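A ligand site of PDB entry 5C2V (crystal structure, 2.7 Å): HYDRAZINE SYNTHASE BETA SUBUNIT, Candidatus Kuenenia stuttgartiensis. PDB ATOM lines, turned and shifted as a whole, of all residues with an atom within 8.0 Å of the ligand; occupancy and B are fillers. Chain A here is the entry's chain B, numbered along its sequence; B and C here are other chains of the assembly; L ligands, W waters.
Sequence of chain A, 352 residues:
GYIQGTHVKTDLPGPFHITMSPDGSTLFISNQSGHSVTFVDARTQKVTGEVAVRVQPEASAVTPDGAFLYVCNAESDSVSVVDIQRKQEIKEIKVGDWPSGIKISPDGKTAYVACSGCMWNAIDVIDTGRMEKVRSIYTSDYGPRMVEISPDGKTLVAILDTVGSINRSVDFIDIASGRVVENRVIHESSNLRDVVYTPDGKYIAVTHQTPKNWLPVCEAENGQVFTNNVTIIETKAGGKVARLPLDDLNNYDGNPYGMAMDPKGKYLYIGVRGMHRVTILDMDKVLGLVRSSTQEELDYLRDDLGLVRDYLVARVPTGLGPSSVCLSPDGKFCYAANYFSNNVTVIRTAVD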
ATOM      1  N   ILE A 166      19.534  -4.073 -33.809  1.00  0.00           N
ATOM      2  CA  ILE A 166      19.285  -3.009 -32.850  1.00  0.00           C
ATOM      3  C   ILE A 166      18.696  -3.577 -31.565  1.00  0.00           C
ATOM      4  O   ILE A 166      19.058  -3.175 -30.470  1.00  0.00           O
ATOM      5  CB  ILE A 166      18.338  -1.947 -33.419  1.00  0.00           C
ATOM      6  CG1 ILE A 166      19.011  -1.229 -34.583  1.00  0.00           C
ATOM      7  CG2 ILE A 166      17.941  -0.948 -32.347  1.00  0.00           C
ATOM      8  CD1 ILE A 166      18.106  -0.247 -35.263  1.00  0.00           C
ATOM      9  N   ASN A 167      17.794  -4.550 -31.720  1.00  0.00           N
ATOM     10  CA  ASN A 167      17.197  -5.169 -30.551  1.00  0.00           C
ATOM     11  C   ASN A 167      17.896  -6.485 -30.278  1.00  0.00           C
ATOM     12  O   ASN A 167      17.750  -7.456 -31.008  1.00  0.00           O
ATOM     13  CB  ASN A 167      15.694  -5.391 -30.765  1.00  0.00           C
ATOM     14  CG  ASN A 167      15.038  -4.222 -31.479  1.00  0.00           C
ATOM     15  OD1 ASN A 167      14.574  -3.269 -30.850  1.00  0.00           O
ATOM     16  ND2 ASN A 167      14.976  -4.301 -32.800  1.00  0.00           N
ATOM     17  N   VAL A 185      13.861  -9.101 -24.888  1.00  0.00           N
ATOM     18  CA  VAL A 185      14.609  -8.166 -25.726  1.00  0.00           C
ATOM     19  C   VAL A 185      14.978  -6.886 -24.988  1.00  0.00           C
ATOM     20  O   VAL A 185      14.119  -6.244 -24.376  1.00  0.00           O
ATOM     21  CB  VAL A 185      13.800  -7.805 -26.992  1.00  0.00           C
ATOM     22  CG1 VAL A 185      14.432  -6.622 -27.705  1.00  0.00           C
ATOM     23  CG2 VAL A 185      13.702  -9.008 -27.913  1.00  0.00           C
ATOM     24  N   ILE A 186      16.251  -6.510 -25.048  1.00  0.00           N
ATOM     25  CA  ILE A 186      16.677  -5.198 -24.590  1.00  0.00           C
ATOM     26  C   ILE A 186      16.637  -4.268 -25.787  1.00  0.00           C
ATOM     27  O   ILE A 186      17.438  -4.413 -26.714  1.00  0.00           O
ATOM     28  CB  ILE A 186      18.091  -5.214 -23.984  1.00  0.00           C
ATOM     29  CG1 ILE A 186      18.166  -6.172 -22.800  1.00  0.00           C
ATOM     30  CG2 ILE A 186      18.495  -3.809 -23.552  1.00  0.00           C
ATOM     31  CD1 ILE A 186      19.530  -6.246 -22.150  1.00  0.00           C
ATOM     32  N   HIS A 187      15.724  -3.312 -25.766  1.00  0.00           N
ATOM     33  CA  HIS A 187      15.504  -2.459 -26.929  1.00  0.00           C
ATOM     34  C   HIS A 187      16.600  -1.420 -27.078  1.00  0.00           C
ATOM     35  O   HIS A 187      17.066  -0.844 -26.091  1.00  0.00           O
ATOM     36  CB  HIS A 187      14.130  -1.785 -26.850  1.00  0.00           C
ATOM     37  CG  HIS A 187      12.995  -2.672 -27.245  1.00  0.00           C
ATOM     38  ND1 HIS A 187      12.649  -3.802 -26.537  1.00  0.00           N
ATOM     39  CD2 HIS A 187      12.136  -2.605 -28.291  1.00  0.00           C
ATOM     40  CE1 HIS A 187      11.629  -4.393 -27.124  1.00  0.00           C
ATOM     41  NE2 HIS A 187      11.291  -3.683 -28.191  1.00  0.00           N
ATOM     42  N   GLU A 188      17.009  -1.185 -28.326  1.00  0.00           N
ATOM     43  CA  GLU A 188      18.057  -0.228 -28.658  1.00  0.00           C
ATOM     44  C   GLU A 188      19.357  -0.527 -27.929  1.00  0.00           C
ATOM     45  O   GLU A 188      19.921   0.345 -27.263  1.00  0.00           O
ATOM     46  CB  GLU A 188      17.591   1.202 -28.350  1.00  0.00           C
ATOM     47  CG  GLU A 188      16.400   1.646 -29.180  1.00  0.00           C
ATOM     48  CD  GLU A 188      16.087   3.124 -29.023  1.00  0.00           C
ATOM     49  OE1 GLU A 188      16.750   3.782 -28.197  1.00  0.00           O
ATOM     50  OE2 GLU A 188      15.191   3.622 -29.732  1.00  0.00           O
ATOM     51  N   THR A 210      23.856   1.860 -25.923  1.00  0.00           N
ATOM     52  CA  THR A 210      22.687   2.288 -26.662  1.00  0.00           C
ATOM     53  C   THR A 210      23.101   3.230 -27.782  1.00  0.00           C
ATOM     54  O   THR A 210      23.475   4.385 -27.540  1.00  0.00           O
ATOM     55  CB  THR A 210      21.674   3.010 -25.746  1.00  0.00           C
ATOM     56  OG1 THR A 210      21.318   2.147 -24.659  1.00  0.00           O
ATOM     57  CG2 THR A 210      20.430   3.407 -26.523  1.00  0.00           C
ATOM     58  N   ARG A 243      16.547  -0.254 -18.346  1.00  0.00           N
ATOM     59  CA  ARG A 243      17.762   0.246 -18.965  1.00  0.00           C
ATOM     60  C   ARG A 243      18.214   1.510 -18.243  1.00  0.00           C
ATOM     61  O   ARG A 243      17.496   2.514 -18.223  1.00  0.00           O
ATOM     62  CB  ARG A 243      17.544   0.522 -20.453  1.00  0.00           C
ATOM     63  CG  ARG A 243      17.104  -0.710 -21.242  1.00  0.00           C
ATOM     64  CD  ARG A 243      16.528  -0.327 -22.598  1.00  0.00           C
ATOM     65  NE  ARG A 243      15.186   0.234 -22.474  1.00  0.00           N
ATOM     66  CZ  ARG A 243      14.522   0.814 -23.472  1.00  0.00           C
ATOM     67  NH1 ARG A 243      15.071   0.907 -24.677  1.00  0.00           N
ATOM     68  NH2 ARG A 243      13.299   1.291 -23.269  1.00  0.00           N
ATOM     69  N   GLN A 295       7.533   0.996 -15.665  1.00  0.00           N
ATOM     70  CA  GLN A 295       8.345   0.749 -16.857  1.00  0.00           C
ATOM     71  C   GLN A 295       8.518   2.043 -17.649  1.00  0.00           C
ATOM     72  O   GLN A 295       9.587   2.322 -18.181  1.00  0.00           O
ATOM     73  CB  GLN A 295       7.709  -0.326 -17.729  1.00  0.00           C
ATOM     74  CG  GLN A 295       8.589  -0.785 -18.885  1.00  0.00           C
ATOM     75  CD  GLN A 295       9.856  -1.483 -18.408  1.00  0.00           C
ATOM     76  OE1 GLN A 295       9.842  -2.674 -18.118  1.00  0.00           O
ATOM     77  NE2 GLN A 295      10.948  -0.736 -18.339  1.00  0.00           N
ATOM     78  N   ASP A 299      11.995   3.926 -18.474  1.00  0.00           N
ATOM     79  CA  ASP A 299      12.308   4.182 -19.868  1.00  0.00           C
ATOM     80  C   ASP A 299      12.637   5.653 -20.092  1.00  0.00           C
ATOM     81  O   ASP A 299      13.485   5.989 -20.920  1.00  0.00           O
ATOM     82  CB  ASP A 299      11.157   3.754 -20.776  1.00  0.00           C
ATOM     83  CG  ASP A 299      11.017   2.247 -20.872  1.00  0.00           C
ATOM     84  OD1 ASP A 299      11.970   1.532 -20.486  1.00  0.00           O
ATOM     85  OD2 ASP A 299       9.948   1.771 -21.324  1.00  0.00           O
ATOM     86  N   ARG A 302      16.166   6.359 -18.473  1.00  0.00           N
ATOM     87  CA  ARG A 302      17.319   5.829 -19.185  1.00  0.00           C
ATOM     88  C   ARG A 302      18.184   6.944 -19.772  1.00  0.00           C
ATOM     89  O   ARG A 302      19.410   6.843 -19.788  1.00  0.00           O
ATOM     90  CB  ARG A 302      16.878   4.878 -20.303  1.00  0.00           C
ATOM     91  CG  ARG A 302      18.022   4.158 -20.996  1.00  0.00           C
ATOM     92  CD  ARG A 302      18.231   4.654 -22.414  1.00  0.00           C
ATOM     93  NE  ARG A 302      17.327   4.015 -23.361  1.00  0.00           N
ATOM     94  CZ  ARG A 302      17.188   4.393 -24.634  1.00  0.00           C
ATOM     95  NH1 ARG A 302      17.897   5.404 -25.104  1.00  0.00           N
ATOM     96  NH2 ARG A 302      16.337   3.761 -25.427  1.00  0.00           N
ATOM     97  N   ASP A 303      17.535   8.008 -20.220  1.00  0.00           N
ATOM     98  CA  ASP A 303      18.222   9.128 -20.853  1.00  0.00           C
ATOM     99  C   ASP A 303      18.566  10.246 -19.864  1.00  0.00           C
ATOM    100  O   ASP A 303      19.091  11.286 -20.265  1.00  0.00           O
ATOM    101  CB  ASP A 303      17.393   9.690 -21.999  1.00  0.00           C
ATOM    102  CG  ASP A 303      17.236   8.707 -23.141  1.00  0.00           C
ATOM    103  OD1 ASP A 303      18.019   7.740 -23.194  1.00  0.00           O
ATOM    104  OD2 ASP A 303      16.344   8.914 -23.983  1.00  0.00           O
ATOM    105  N   GLY B 240       9.621   3.711 -39.428  1.00  0.00           N
ATOM    106  CA  GLY B 240       9.671   2.958 -38.182  1.00  0.00           C
ATOM    107  C   GLY B 240      11.023   2.963 -37.485  1.00  0.00           C
ATOM    108  O   GLY B 240      12.070   2.876 -38.137  1.00  0.00           O
ATOM    109  N   VAL B 241      11.009   3.076 -36.159  1.00  0.00           N
ATOM    110  CA  VAL B 241      12.236   3.153 -35.365  1.00  0.00           C
ATOM    111  C   VAL B 241      12.680   1.811 -34.790  1.00  0.00           C
ATOM    112  O   VAL B 241      13.767   1.695 -34.222  1.00  0.00           O
ATOM    113  CB  VAL B 241      12.059   4.174 -34.211  1.00  0.00           C
ATOM    114  CG1 VAL B 241      11.332   3.517 -33.037  1.00  0.00           C
ATOM    115  CG2 VAL B 241      13.394   4.747 -33.759  1.00  0.00           C
ATOM    116  N   GLU B 242      11.849   0.775 -34.946  1.00  0.00           N
ATOM    117  CA  GLU B 242      12.128  -0.525 -34.340  1.00  0.00           C
ATOM    118  C   GLU B 242      12.844  -1.493 -35.277  1.00  0.00           C
ATOM    119  O   GLU B 242      13.281  -2.565 -34.854  1.00  0.00           O
ATOM    120  CB  GLU B 242      10.833  -1.157 -33.844  1.00  0.00           C
ATOM    121  CG  GLU B 242      10.463  -0.757 -32.418  1.00  0.00           C
ATOM    122  CD  GLU B 242       9.025  -1.085 -32.084  1.00  0.00           C
ATOM    123  OE1 GLU B 242       8.137  -0.807 -32.916  1.00  0.00           O
ATOM    124  OE2 GLU B 242       8.771  -1.629 -30.988  1.00  0.00           O
ATOM    125  N   SER B 243      12.968  -1.119 -36.543  1.00  0.00           N
ATOM    126  CA  SER B 243      13.571  -1.994 -37.547  1.00  0.00           C
ATOM    127  C   SER B 243      15.083  -2.103 -37.368  1.00  0.00           C
ATOM    128  O   SER B 243      15.745  -1.131 -37.031  1.00  0.00           O
ATOM    129  CB  SER B 243      13.253  -1.497 -38.953  1.00  0.00           C
ATOM    130  OG  SER B 243      11.850  -1.336 -39.137  1.00  0.00           O
ATOM    131  N   LYS C 570      17.139  11.525 -28.156  1.00  0.00           N
ATOM    132  CA  LYS C 570      16.154  10.471 -28.343  1.00  0.00           C
ATOM    133  C   LYS C 570      16.310   9.858 -29.725  1.00  0.00           C
ATOM    134  O   LYS C 570      16.522  10.584 -30.706  1.00  0.00           O
ATOM    135  CB  LYS C 570      14.738  11.021 -28.161  1.00  0.00           C
ATOM    136  CG  LYS C 570      13.643   9.975 -28.254  1.00  0.00           C
ATOM    137  CD  LYS C 570      12.279  10.595 -27.995  1.00  0.00           C
ATOM    138  CE  LYS C 570      11.190   9.540 -27.984  1.00  0.00           C
ATOM    139  NZ  LYS C 570       9.852  10.133 -27.741  1.00  0.00           N
ATOM    140  N   ASN C 571      16.211   8.539 -29.815  1.00  0.00           N
ATOM    141  CA  ASN C 571      16.338   7.898 -31.117  1.00  0.00           C
ATOM    142  C   ASN C 571      15.035   8.083 -31.870  1.00  0.00           C
ATOM    143  O   ASN C 571      13.991   7.581 -31.475  1.00  0.00           O
ATOM    144  CB  ASN C 571      16.673   6.418 -30.964  1.00  0.00           C
ATOM    145  CG  ASN C 571      17.204   5.802 -32.246  1.00  0.00           C
ATOM    146  OD1 ASN C 571      17.790   6.488 -33.088  1.00  0.00           O
ATOM    147  ND2 ASN C 571      17.005   4.493 -32.404  1.00  0.00           N
HETATM  148  N1  LIG L   1      10.639   1.772 -28.424  1.00  0.00           N
HETATM  149  C1  LIG L   1      12.150   1.563 -28.317  1.00  0.00           C
HETATM  150  C2  LIG L   1      12.639   1.875 -26.805  1.00  0.00           C
HETATM  151  O1  LIG L   1      13.355   2.904 -26.710  1.00  0.00           O
HETATM  152  O2  LIG L   1      12.251   1.043 -25.949  1.00  0.00           O
HETATM  153  C3  LIG L   1      10.255   2.104 -29.851  1.00  0.00           C
HETATM  154  C4  LIG L   1      10.177   2.926 -27.531  1.00  0.00           C
HETATM  155  C5  LIG L   1       9.910   0.485 -28.079  1.00  0.00           C
HETATM  156  O   HOH W   1      13.322   4.550 -24.532  1.00  0.00           O
HETATM  157  O   HOH W   2      13.913   1.705 -31.310  1.00  0.00           O
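An oxygen (O1) of the ligand is in salt-bridge range of the guanidinium group (NH2) of Arg 302 (3.4 Å). O2 of the ligand is in salt-bridge range of NH2 of Arg 243 of chain A (2.9 Å).
The backbone carbonyl oxygen (O) of Glu 242 of chain B sits at hydrogen-bond distance from the side-chain amide nitrogen (ND2) of Asn 167 (3.2 Å). O of Glu 188 sits close to OG1 of Thr 210 (3.5 Å). NH1 of Arg 243 of chain A is in hydrogen-bond range of O of His 187. The side-chain carboxylate (OE2) of Glu 188 is in hydrogen-bond range of the side-chain amide nitrogen (ND2) of Asn 571 of chain C (3.3 Å). The guanidinium group of Arg 243 of chain A is in salt-bridge range of the side-chain carboxylate of Asp 299, 3.1 Å away. The guanidinium group of Arg 302 lies within salt-bridge range of the side-chain carboxylate of Asp 303, 3.0 Å away. NH2 of Arg 302 lies within salt-bridge range of OE1 of Glu 188 (2.8 Å).
Residues that only touch the ligand: His 187 (3.5 Å), Glu 188 (3.6 Å), Val 241 of chain B (3.6 Å) and Glu 242 of chain B (3.8 Å). Six residues have an atom within 4 Å of the ligand: His 187, Glu 188, Arg 243 of chain A, Arg 302, Val 241 of chain B and Glu 242 of chain B.
Water W1 lies within hydrogen-bond range of an oxygen (O1) of the ligand (2.7 Å), the guanidinium group (NH2) of Arg 302 (3.2 Å) and the guanidinium group (NH2) of Arg 243 of chain A (3.5 Å). Water W2 lies within hydrogen-bond range of the side-chain carboxylate of Glu 188 (2.8 Å) and the backbone carbonyl oxygen of Val 241 of chain B (2.9 Å).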
